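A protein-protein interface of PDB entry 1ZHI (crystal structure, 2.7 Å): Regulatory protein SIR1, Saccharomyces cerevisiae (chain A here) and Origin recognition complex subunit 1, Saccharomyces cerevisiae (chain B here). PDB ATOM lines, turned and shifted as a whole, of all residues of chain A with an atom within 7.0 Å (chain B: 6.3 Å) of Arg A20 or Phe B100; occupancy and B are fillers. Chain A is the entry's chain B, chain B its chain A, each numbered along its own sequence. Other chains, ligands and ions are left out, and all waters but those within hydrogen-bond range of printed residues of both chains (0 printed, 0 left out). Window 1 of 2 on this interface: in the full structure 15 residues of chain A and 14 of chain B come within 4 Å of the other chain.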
ATOM      1  N   TYR A  16      38.514   9.987 -19.348  1.00  0.00           N
ATOM      2  CA  TYR A  16      37.153   9.964 -18.819  1.00  0.00           C
ATOM      3  C   TYR A  16      36.177  10.216 -19.941  1.00  0.00           C
ATOM      4  O   TYR A  16      35.808  11.352 -20.204  1.00  0.00           O
ATOM      5  CB  TYR A  16      36.980  11.058 -17.775  1.00  0.00           C
ATOM      6  CG  TYR A  16      37.430  10.693 -16.385  1.00  0.00           C
ATOM      7  CD1 TYR A  16      38.755  10.846 -15.995  1.00  0.00           C
ATOM      8  CD2 TYR A  16      36.519  10.224 -15.447  1.00  0.00           C
ATOM      9  CE1 TYR A  16      39.157  10.528 -14.717  1.00  0.00           C
ATOM     10  CE2 TYR A  16      36.912   9.906 -14.166  1.00  0.00           C
ATOM     11  CZ  TYR A  16      38.223  10.054 -13.804  1.00  0.00           C
ATOM     12  OH  TYR A  16      38.604   9.731 -12.518  1.00  0.00           O
ATOM     13  N   VAL A  17      35.747   9.153 -20.596  1.00  0.00           N
ATOM     14  CA  VAL A  17      34.961   9.286 -21.802  1.00  0.00           C
ATOM     15  C   VAL A  17      33.525   9.727 -21.485  1.00  0.00           C
ATOM     16  O   VAL A  17      32.821  10.260 -22.351  1.00  0.00           O
ATOM     17  CB  VAL A  17      35.036   7.987 -22.701  1.00  0.00           C
ATOM     18  CG1 VAL A  17      36.490   7.573 -22.914  1.00  0.00           C
ATOM     19  CG2 VAL A  17      34.244   6.826 -22.103  1.00  0.00           C
ATOM     20  N   SER A  18      33.110   9.507 -20.239  1.00  0.00           N
ATOM     21  CA  SER A  18      31.894  10.110 -19.682  1.00  0.00           C
ATOM     22  C   SER A  18      32.124  10.208 -18.181  1.00  0.00           C
ATOM     23  O   SER A  18      33.173   9.763 -17.708  1.00  0.00           O
ATOM     24  CB  SER A  18      30.658   9.262 -20.010  1.00  0.00           C
ATOM     25  OG  SER A  18      30.755   7.943 -19.479  1.00  0.00           O
ATOM     26  N   PRO A  19      31.190  10.783 -17.416  1.00  0.00           N
ATOM     27  CA  PRO A  19      31.344  10.814 -15.948  1.00  0.00           C
ATOM     28  C   PRO A  19      31.337   9.398 -15.322  1.00  0.00           C
ATOM     29  O   PRO A  19      31.905   9.218 -14.240  1.00  0.00           O
ATOM     30  CB  PRO A  19      30.137  11.640 -15.476  1.00  0.00           C
ATOM     31  CG  PRO A  19      29.681  12.377 -16.690  1.00  0.00           C
ATOM     32  CD  PRO A  19      29.958  11.457 -17.848  1.00  0.00           C
ATOM     33  N   ARG A  20      30.748   8.414 -16.006  1.00  0.00           N
ATOM     34  CA  ARG A  20      30.709   7.058 -15.468  1.00  0.00           C
ATOM     35  C   ARG A  20      31.919   6.235 -15.871  1.00  0.00           C
ATOM     36  O   ARG A  20      32.382   5.383 -15.102  1.00  0.00           O
ATOM     37  CB  ARG A  20      29.434   6.331 -15.903  1.00  0.00           C
ATOM     38  CG  ARG A  20      29.281   4.957 -15.297  1.00  0.00           C
ATOM     39  CD  ARG A  20      27.929   4.350 -15.567  1.00  0.00           C
ATOM     40  NE  ARG A  20      27.801   2.981 -15.076  1.00  0.00           N
ATOM     41  CZ  ARG A  20      26.713   2.252 -15.236  1.00  0.00           C
ATOM     42  NH1 ARG A  20      25.659   2.772 -15.878  1.00  0.00           N
ATOM     43  NH2 ARG A  20      26.667   1.001 -14.761  1.00  0.00           N
ATOM     44  N   PHE A  21      32.421   6.483 -17.079  1.00  0.00           N
ATOM     45  CA  PHE A  21      33.347   5.556 -17.705  1.00  0.00           C
ATOM     46  C   PHE A  21      34.751   6.090 -17.863  1.00  0.00           C
ATOM     47  O   PHE A  21      34.979   7.137 -18.489  1.00  0.00           O
ATOM     48  CB  PHE A  21      32.788   5.037 -19.030  1.00  0.00           C
ATOM     49  CG  PHE A  21      31.615   4.115 -18.855  1.00  0.00           C
ATOM     50  CD1 PHE A  21      30.342   4.484 -19.311  1.00  0.00           C
ATOM     51  CD2 PHE A  21      31.769   2.883 -18.188  1.00  0.00           C
ATOM     52  CE1 PHE A  21      29.258   3.651 -19.126  1.00  0.00           C
ATOM     53  CE2 PHE A  21      30.678   2.037 -18.010  1.00  0.00           C
ATOM     54  CZ  PHE A  21      29.416   2.424 -18.476  1.00  0.00           C
ATOM     55  N   LEU A  22      35.687   5.350 -17.272  1.00  0.00           N
ATOM     56  CA  LEU A  22      37.090   5.705 -17.270  1.00  0.00           C
ATOM     57  C   LEU A  22      37.812   4.698 -18.117  1.00  0.00           C
ATOM     58  O   LEU A  22      37.650   3.493 -17.925  1.00  0.00           O
ATOM     59  CB  LEU A  22      37.648   5.646 -15.843  1.00  0.00           C
ATOM     60  CG  LEU A  22      38.853   6.473 -15.385  1.00  0.00           C
ATOM     61  CD1 LEU A  22      39.376   5.890 -14.120  1.00  0.00           C
ATOM     62  CD2 LEU A  22      39.962   6.543 -16.396  1.00  0.00           C
ATOM     63  N   ILE A  29      36.674   1.134 -17.196  1.00  0.00           N
ATOM     64  CA  ILE A  29      36.323   1.097 -15.786  1.00  0.00           C
ATOM     65  C   ILE A  29      34.990   1.784 -15.571  1.00  0.00           C
ATOM     66  O   ILE A  29      34.839   2.966 -15.886  1.00  0.00           O
ATOM     67  CB  ILE A  29      37.421   1.801 -14.941  1.00  0.00           C
ATOM     68  CG1 ILE A  29      38.720   1.005 -14.973  1.00  0.00           C
ATOM     69  CG2 ILE A  29      36.965   2.036 -13.499  1.00  0.00           C
ATOM     70  CD1 ILE A  29      39.944   1.847 -14.618  1.00  0.00           C
ATOM     71  N   ASP A  30      34.037   1.036 -15.009  1.00  0.00           N
ATOM     72  CA  ASP A  30      32.700   1.532 -14.678  1.00  0.00           C
ATOM     73  C   ASP A  30      32.737   2.073 -13.269  1.00  0.00           C
ATOM     74  O   ASP A  30      32.821   1.304 -12.306  1.00  0.00           O
ATOM     75  CB  ASP A  30      31.715   0.364 -14.768  1.00  0.00           C
ATOM     76  CG  ASP A  30      30.282   0.748 -14.427  1.00  0.00           C
ATOM     77  OD1 ASP A  30      30.039   1.837 -13.830  1.00  0.00           O
ATOM     78  OD2 ASP A  30      29.324  -0.019 -14.708  1.00  0.00           O
ATOM     79  N   LEU A  31      32.674   3.391 -13.131  1.00  0.00           N
ATOM     80  CA  LEU A  31      32.956   4.020 -11.832  1.00  0.00           C
ATOM     81  C   LEU A  31      31.781   4.001 -10.855  1.00  0.00           C
ATOM     82  O   LEU A  31      31.951   4.323  -9.681  1.00  0.00           O
ATOM     83  CB  LEU A  31      33.478   5.450 -12.003  1.00  0.00           C
ATOM     84  CG  LEU A  31      34.796   5.737 -12.746  1.00  0.00           C
ATOM     85  CD1 LEU A  31      34.877   7.216 -13.097  1.00  0.00           C
ATOM     86  CD2 LEU A  31      35.988   5.352 -11.946  1.00  0.00           C
ATOM     87  N   ALA A  32      30.590   3.637 -11.337  1.00  0.00           N
ATOM     88  CA  ALA A  32      29.436   3.417 -10.455  1.00  0.00           C
ATOM     89  C   ALA A  32      29.557   2.078  -9.718  1.00  0.00           C
ATOM     90  O   ALA A  32      29.244   1.981  -8.524  1.00  0.00           O
ATOM     91  CB  ALA A  32      28.170   3.460 -11.239  1.00  0.00           C
ATOM     92  N   GLU A  33      30.032   1.058 -10.437  1.00  0.00           N
ATOM     93  CA  GLU A  33      30.158  -0.305  -9.907  1.00  0.00           C
ATOM     94  C   GLU A  33      31.558  -0.576  -9.398  1.00  0.00           C
ATOM     95  O   GLU A  33      31.802  -1.590  -8.757  1.00  0.00           O
ATOM     96  CB  GLU A  33      29.797  -1.340 -10.980  1.00  0.00           C
ATOM     97  CG  GLU A  33      28.334  -1.361 -11.369  1.00  0.00           C
ATOM     98  CD  GLU A  33      27.438  -1.840 -10.244  1.00  0.00           C
ATOM     99  OE1 GLU A  33      27.490  -3.055  -9.907  1.00  0.00           O
ATOM    100  OE2 GLU A  33      26.676  -1.003  -9.700  1.00  0.00           O
ATOM    101  N   ILE A  37      34.753  -3.315 -17.195  1.00  0.00           N
ATOM    102  CA  ILE A  37      33.695  -3.804 -18.076  1.00  0.00           C
ATOM    103  C   ILE A  37      34.315  -4.271 -19.361  1.00  0.00           C
ATOM    104  O   ILE A  37      35.112  -3.556 -19.963  1.00  0.00           O
ATOM    105  CB  ILE A  37      32.719  -2.653 -18.423  1.00  0.00           C
ATOM    106  CG1 ILE A  37      32.124  -2.050 -17.180  1.00  0.00           C
ATOM    107  CG2 ILE A  37      31.551  -3.142 -19.319  1.00  0.00           C
ATOM    108  CD1 ILE A  37      31.231  -0.885 -17.507  1.00  0.00           C
ATOM    109  N   ARG A  43      25.650  -4.265 -22.903  1.00  0.00           N
ATOM    110  CA  ARG A  43      25.060  -3.205 -22.083  1.00  0.00           C
ATOM    111  C   ARG A  43      25.506  -1.788 -22.472  1.00  0.00           C
ATOM    112  O   ARG A  43      24.826  -0.812 -22.167  1.00  0.00           O
ATOM    113  CB  ARG A  43      25.414  -3.436 -20.637  1.00  0.00           C
ATOM    114  CG  ARG A  43      24.284  -3.163 -19.677  1.00  0.00           C
ATOM    115  CD  ARG A  43      24.758  -3.095 -18.226  1.00  0.00           C
ATOM    116  NE  ARG A  43      24.904  -4.394 -17.568  1.00  0.00           N
ATOM    117  CZ  ARG A  43      23.898  -5.141 -17.241  1.00  0.00           C
ATOM    118  NH1 ARG A  43      22.682  -4.760 -17.561  1.00  0.00           N
ATOM    119  NH2 ARG A  43      24.091  -6.282 -16.604  1.00  0.00           N
ATOM    120  N   LEU A  47      24.177   2.371 -22.778  1.00  0.00           N
ATOM    121  CA  LEU A  47      24.743   3.407 -21.934  1.00  0.00           C
ATOM    122  C   LEU A  47      25.551   4.493 -22.673  1.00  0.00           C
ATOM    123  O   LEU A  47      25.547   5.653 -22.248  1.00  0.00           O
ATOM    124  CB  LEU A  47      25.595   2.792 -20.804  1.00  0.00           C
ATOM    125  CG  LEU A  47      24.931   1.713 -19.924  1.00  0.00           C
ATOM    126  CD1 LEU A  47      25.963   1.090 -18.973  1.00  0.00           C
ATOM    127  CD2 LEU A  47      23.731   2.262 -19.158  1.00  0.00           C
ATOM    128  N   ALA B  68      19.121  -2.661 -16.701  1.00  0.00           N
ATOM    129  CA  ALA B  68      19.512  -2.085 -17.988  1.00  0.00           C
ATOM    130  C   ALA B  68      20.693  -1.133 -17.820  1.00  0.00           C
ATOM    131  O   ALA B  68      21.585  -1.068 -18.670  1.00  0.00           O
ATOM    132  CB  ALA B  68      18.353  -1.363 -18.621  1.00  0.00           C
ATOM    133  N   ALA B  69      20.690  -0.392 -16.719  1.00  0.00           N
ATOM    134  CA  ALA B  69      21.790   0.504 -16.409  1.00  0.00           C
ATOM    135  C   ALA B  69      23.023  -0.244 -15.853  1.00  0.00           C
ATOM    136  O   ALA B  69      24.121   0.300 -15.871  1.00  0.00           O
ATOM    137  CB  ALA B  69      21.339   1.552 -15.454  1.00  0.00           C
ATOM    138  N   GLY B  70      22.839  -1.484 -15.381  1.00  0.00           N
ATOM    139  CA  GLY B  70      23.931  -2.249 -14.805  1.00  0.00           C
ATOM    140  C   GLY B  70      24.410  -1.714 -13.462  1.00  0.00           C
ATOM    141  O   GLY B  70      25.511  -2.019 -13.036  1.00  0.00           O
ATOM    142  N   THR B  71      23.576  -0.906 -12.806  1.00  0.00           N
ATOM    143  CA  THR B  71      23.882  -0.307 -11.511  1.00  0.00           C
ATOM    144  C   THR B  71      22.529   0.026 -10.869  1.00  0.00           C
ATOM    145  O   THR B  71      21.497  -0.180 -11.498  1.00  0.00           O
ATOM    146  CB  THR B  71      24.770   0.953 -11.700  1.00  0.00           C
ATOM    147  OG1 THR B  71      25.212   1.449 -10.422  1.00  0.00           O
ATOM    148  CG2 THR B  71      23.978   2.112 -12.318  1.00  0.00           C
ATOM    149  N   TYR B  72      22.501   0.499  -9.631  1.00  0.00           N
ATOM    150  CA  TYR B  72      21.212   0.695  -8.960  1.00  0.00           C
ATOM    151  C   TYR B  72      20.672   2.087  -9.214  1.00  0.00           C
ATOM    152  O   TYR B  72      21.424   3.007  -9.554  1.00  0.00           O
ATOM    153  CB  TYR B  72      21.319   0.421  -7.440  1.00  0.00           C
ATOM    154  CG  TYR B  72      22.110   1.451  -6.675  1.00  0.00           C
ATOM    155  CD1 TYR B  72      21.551   2.693  -6.360  1.00  0.00           C
ATOM    156  CD2 TYR B  72      23.420   1.188  -6.262  1.00  0.00           C
ATOM    157  CE1 TYR B  72      22.272   3.655  -5.661  1.00  0.00           C
ATOM    158  CE2 TYR B  72      24.165   2.144  -5.530  1.00  0.00           C
ATOM    159  CZ  TYR B  72      23.577   3.380  -5.241  1.00  0.00           C
ATOM    160  OH  TYR B  72      24.269   4.342  -4.533  1.00  0.00           O
ATOM    161  N   LEU B  97      18.392  11.256 -10.214  1.00  0.00           N
ATOM    162  CA  LEU B  97      19.654  11.094 -10.941  1.00  0.00           C
ATOM    163  C   LEU B  97      20.776  10.845  -9.950  1.00  0.00           C
ATOM    164  O   LEU B  97      20.828  11.460  -8.853  1.00  0.00           O
ATOM    165  CB  LEU B  97      19.989  12.340 -11.751  1.00  0.00           C
ATOM    166  CG  LEU B  97      19.098  12.754 -12.918  1.00  0.00           C
ATOM    167  CD1 LEU B  97      19.784  13.839 -13.719  1.00  0.00           C
ATOM    168  CD2 LEU B  97      18.684  11.589 -13.822  1.00  0.00           C
ATOM    169  N   ARG B  98      21.672   9.944 -10.314  1.00  0.00           N
ATOM    170  CA  ARG B  98      22.918   9.814  -9.595  1.00  0.00           C
ATOM    171  C   ARG B  98      23.977  10.629 -10.296  1.00  0.00           C
ATOM    172  O   ARG B  98      23.817  11.044 -11.445  1.00  0.00           O
ATOM    173  CB  ARG B  98      23.345   8.364  -9.505  1.00  0.00           C
ATOM    174  CG  ARG B  98      22.603   7.585  -8.457  1.00  0.00           C
ATOM    175  CD  ARG B  98      22.795   6.135  -8.569  1.00  0.00           C
ATOM    176  NE  ARG B  98      24.107   5.743  -8.077  1.00  0.00           N
ATOM    177  CZ  ARG B  98      24.683   4.589  -8.350  1.00  0.00           C
ATOM    178  NH1 ARG B  98      24.080   3.707  -9.133  1.00  0.00           N
ATOM    179  NH2 ARG B  98      25.870   4.320  -7.845  1.00  0.00           N
ATOM    180  N   TRP B  99      25.078  10.831  -9.599  1.00  0.00           N
ATOM    181  CA  TRP B  99      26.095  11.774 -10.015  1.00  0.00           C
ATOM    182  C   TRP B  99      26.534  11.586 -11.469  1.00  0.00           C
ATOM    183  O   TRP B  99      26.745  12.565 -12.185  1.00  0.00           O
ATOM    184  CB  TRP B  99      27.297  11.684  -9.065  1.00  0.00           C
ATOM    185  CG  TRP B  99      27.954  10.331  -9.057  1.00  0.00           C
ATOM    186  CD1 TRP B  99      27.592   9.232  -8.308  1.00  0.00           C
ATOM    187  CD2 TRP B  99      29.091   9.929  -9.832  1.00  0.00           C
ATOM    188  NE1 TRP B  99      28.447   8.183  -8.562  1.00  0.00           N
ATOM    189  CE2 TRP B  99      29.374   8.576  -9.496  1.00  0.00           C
ATOM    190  CE3 TRP B  99      29.913  10.577 -10.778  1.00  0.00           C
ATOM    191  CZ2 TRP B  99      30.435   7.858 -10.078  1.00  0.00           C
ATOM    192  CZ3 TRP B  99      30.969   9.867 -11.351  1.00  0.00           C
ATOM    193  CH2 TRP B  99      31.220   8.518 -10.998  1.00  0.00           C
ATOM    194  N   PHE B 100      26.672  10.339 -11.899  1.00  0.00           N
ATOM    195  CA  PHE B 100      27.216  10.040 -13.235  1.00  0.00           C
ATOM    196  C   PHE B 100      26.211  10.306 -14.366  1.00  0.00           C
ATOM    197  O   PHE B 100      26.557  10.216 -15.540  1.00  0.00           O
ATOM    198  CB  PHE B 100      27.723   8.585 -13.302  1.00  0.00           C
ATOM    199  CG  PHE B 100      26.688   7.567 -12.896  1.00  0.00           C
ATOM    200  CD1 PHE B 100      25.806   7.044 -13.835  1.00  0.00           C
ATOM    201  CD2 PHE B 100      26.577   7.168 -11.563  1.00  0.00           C
ATOM    202  CE1 PHE B 100      24.824   6.127 -13.461  1.00  0.00           C
ATOM    203  CE2 PHE B 100      25.620   6.262 -11.179  1.00  0.00           C
ATOM    204  CZ  PHE B 100      24.725   5.726 -12.143  1.00  0.00           C
ATOM    205  N   GLU B 101      24.974  10.625 -13.997  1.00  0.00           N
ATOM    206  CA  GLU B 101      23.921  10.940 -14.956  1.00  0.00           C
ATOM    207  C   GLU B 101      23.744  12.465 -15.120  1.00  0.00           C
ATOM    208  O   GLU B 101      22.879  12.932 -15.869  1.00  0.00           O
ATOM    209  CB  GLU B 101      22.598  10.302 -14.521  1.00  0.00           C
ATOM    210  CG  GLU B 101      22.643   8.789 -14.371  1.00  0.00           C
ATOM    211  CD  GLU B 101      21.374   8.231 -13.757  1.00  0.00           C
ATOM    212  OE1 GLU B 101      21.236   8.250 -12.511  1.00  0.00           O
ATOM    213  OE2 GLU B 101      20.516   7.765 -14.516  1.00  0.00           O
ATOM    214  N   VAL B 102      24.550  13.230 -14.392  1.00  0.00           N
ATOM    215  CA  VAL B 102      24.621  14.675 -14.573  1.00  0.00           C
ATOM    216  C   VAL B 102      25.307  14.993 -15.906  1.00  0.00           C
ATOM    217  O   VAL B 102      26.210  14.273 -16.328  1.00  0.00           O
ATOM    218  CB  VAL B 102      25.374  15.355 -13.391  1.00  0.00           C
ATOM    219  CG1 VAL B 102      25.829  16.767 -13.743  1.00  0.00           C
ATOM    220  CG2 VAL B 102      24.492  15.373 -12.150  1.00  0.00           C
ATOM    221  N   ASN B 103      24.839  16.044 -16.580  1.00  0.00           N
ATOM    222  CA  ASN B 103      25.545  16.598 -17.723  1.00  0.00           C
ATOM    223  C   ASN B 103      26.586  17.603 -17.220  1.00  0.00           C
ATOM    224  O   ASN B 103      26.260  18.758 -16.894  1.00  0.00           O
ATOM    225  CB  ASN B 103      24.566  17.251 -18.696  1.00  0.00           C
ATOM    226  CG  ASN B 103      25.260  17.879 -19.913  1.00  0.00           C
ATOM    227  OD1 ASN B 103      26.422  18.301 -19.848  1.00  0.00           O
ATOM    228  ND2 ASN B 103      24.529  17.966 -21.023  1.00  0.00           N
ATOM    229  N   PHE B 129      33.918  16.548 -12.774  1.00  0.00           N
ATOM    230  CA  PHE B 129      32.697  16.180 -12.066  1.00  0.00           C
ATOM    231  C   PHE B 129      32.839  14.866 -11.296  1.00  0.00           C
ATOM    232  O   PHE B 129      32.593  14.811 -10.092  1.00  0.00           O
ATOM    233  CB  PHE B 129      31.463  16.168 -12.967  1.00  0.00           C
ATOM    234  CG  PHE B 129      30.176  16.378 -12.213  1.00  0.00           C
ATOM    235  CD1 PHE B 129      29.761  17.667 -11.861  1.00  0.00           C
ATOM    236  CD2 PHE B 129      29.409  15.291 -11.805  1.00  0.00           C
ATOM    237  CE1 PHE B 129      28.585  17.868 -11.144  1.00  0.00           C
ATOM    238  CE2 PHE B 129      28.243  15.477 -11.082  1.00  0.00           C
ATOM    239  CZ  PHE B 129      27.822  16.769 -10.753  1.00  0.00           C
ATOM    240  N   SER B 130      33.269  13.825 -11.983  1.00  0.00           N
ATOM    241  CA  SER B 130      33.498  12.538 -11.339  1.00  0.00           C
ATOM    242  C   SER B 130      34.388  12.641 -10.073  1.00  0.00           C
ATOM    243  O   SER B 130      34.198  11.891  -9.110  1.00  0.00           O
ATOM    244  CB  SER B 130      34.087  11.544 -12.345  1.00  0.00           C
ATOM    245  OG  SER B 130      34.820  10.532 -11.691  1.00  0.00           O
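Hydrophobic or aromatic side chains of chain B that line the printed part of chain A: Trp B99 and Phe B100.
Of the 15 printed residues of chain A, 8 touch a printed residue of chain B.
Hydrophobic or aromatic side chains of chain A that line the printed part of chain B: Tyr A16, Pro A19, Leu A31, Ala A32 and Leu A47.
Among the printed residues, 19 pairs touch across the chains.
Among the printed residues, no Asp or Glu carboxylate lies within 4 Å of a Lys or Arg side-chain nitrogen of the other chain.
Of the printed residues of chain B, Tyr A16 touches Ser B130.
Leu A22 touches none of the printed residues of chain B.
Ile A29 touches none of the printed residues of chain B.
Of the printed residues of chain A, Thr B71 touches Arg A20, Ala A32 and Glu A33.
Of chain A, only Pro A19 (3.9 Å), Arg A20 (3.8 Å) and Ala A32 (3.8 Å) come within 4 Å of Phe B100.
The nearest residue of chain B that does not touch Arg A20 is Trp B99 (4.7 Å).
Tyr A16 touches Ser B130 (CE2 to OG, 3.3 Å).
O of Val B102 touches CG of Pro A19, 3.97 Å away.
CB of Ser B130 touches O of Pro A19, at 3.7 Å.
NH2 of Arg A20 touches O of Gly B70, at 3.7 Å.
CD1 of Leu A31 touches OG of Ser B130, at 3.6 Å.
CB of Ala A32 touches OG1 of Thr B71, 3.7 Å away.
Gly B70 touches Glu A33.
Arg A43 touches Gly B70.
O of Ala B68 touches CD2 of Leu A47 (3.99 Å).
Leu A47 touches Ala B69.
OG1 of Thr B71 sits at hydrogen-bond distance from NH1 of Arg B98 (2.8 Å).
The guanidinium group (NE) of Arg A20 lies within salt-bridge range of the side-chain carboxylate (OD1) of Asp A30, 2.8 Å away.
The backbone carbonyl oxygen of Arg A20 lies within hydrogen-bond range of the backbone NH of Leu A31 (2.8 Å).
OD1 of Asp A30 lies within hydrogen-bond range of N of Ala A32 (3.1 Å).
The backbone NH (N) of Glu A33 sits at hydrogen-bond distance from the side-chain carboxylate (OD1) of Asp A30, at 3.5 Å.
The backbone carbonyl oxygen (O) of Ala B69 sits at hydrogen-bond distance from the guanidinium group (NH2) of Arg A20, at 2.9 Å.
The side-chain hydroxyl (OG1) of Thr B71 is in hydrogen-bond range of the side-chain carboxylate (OE2) of Glu A33 (2.9 Å).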
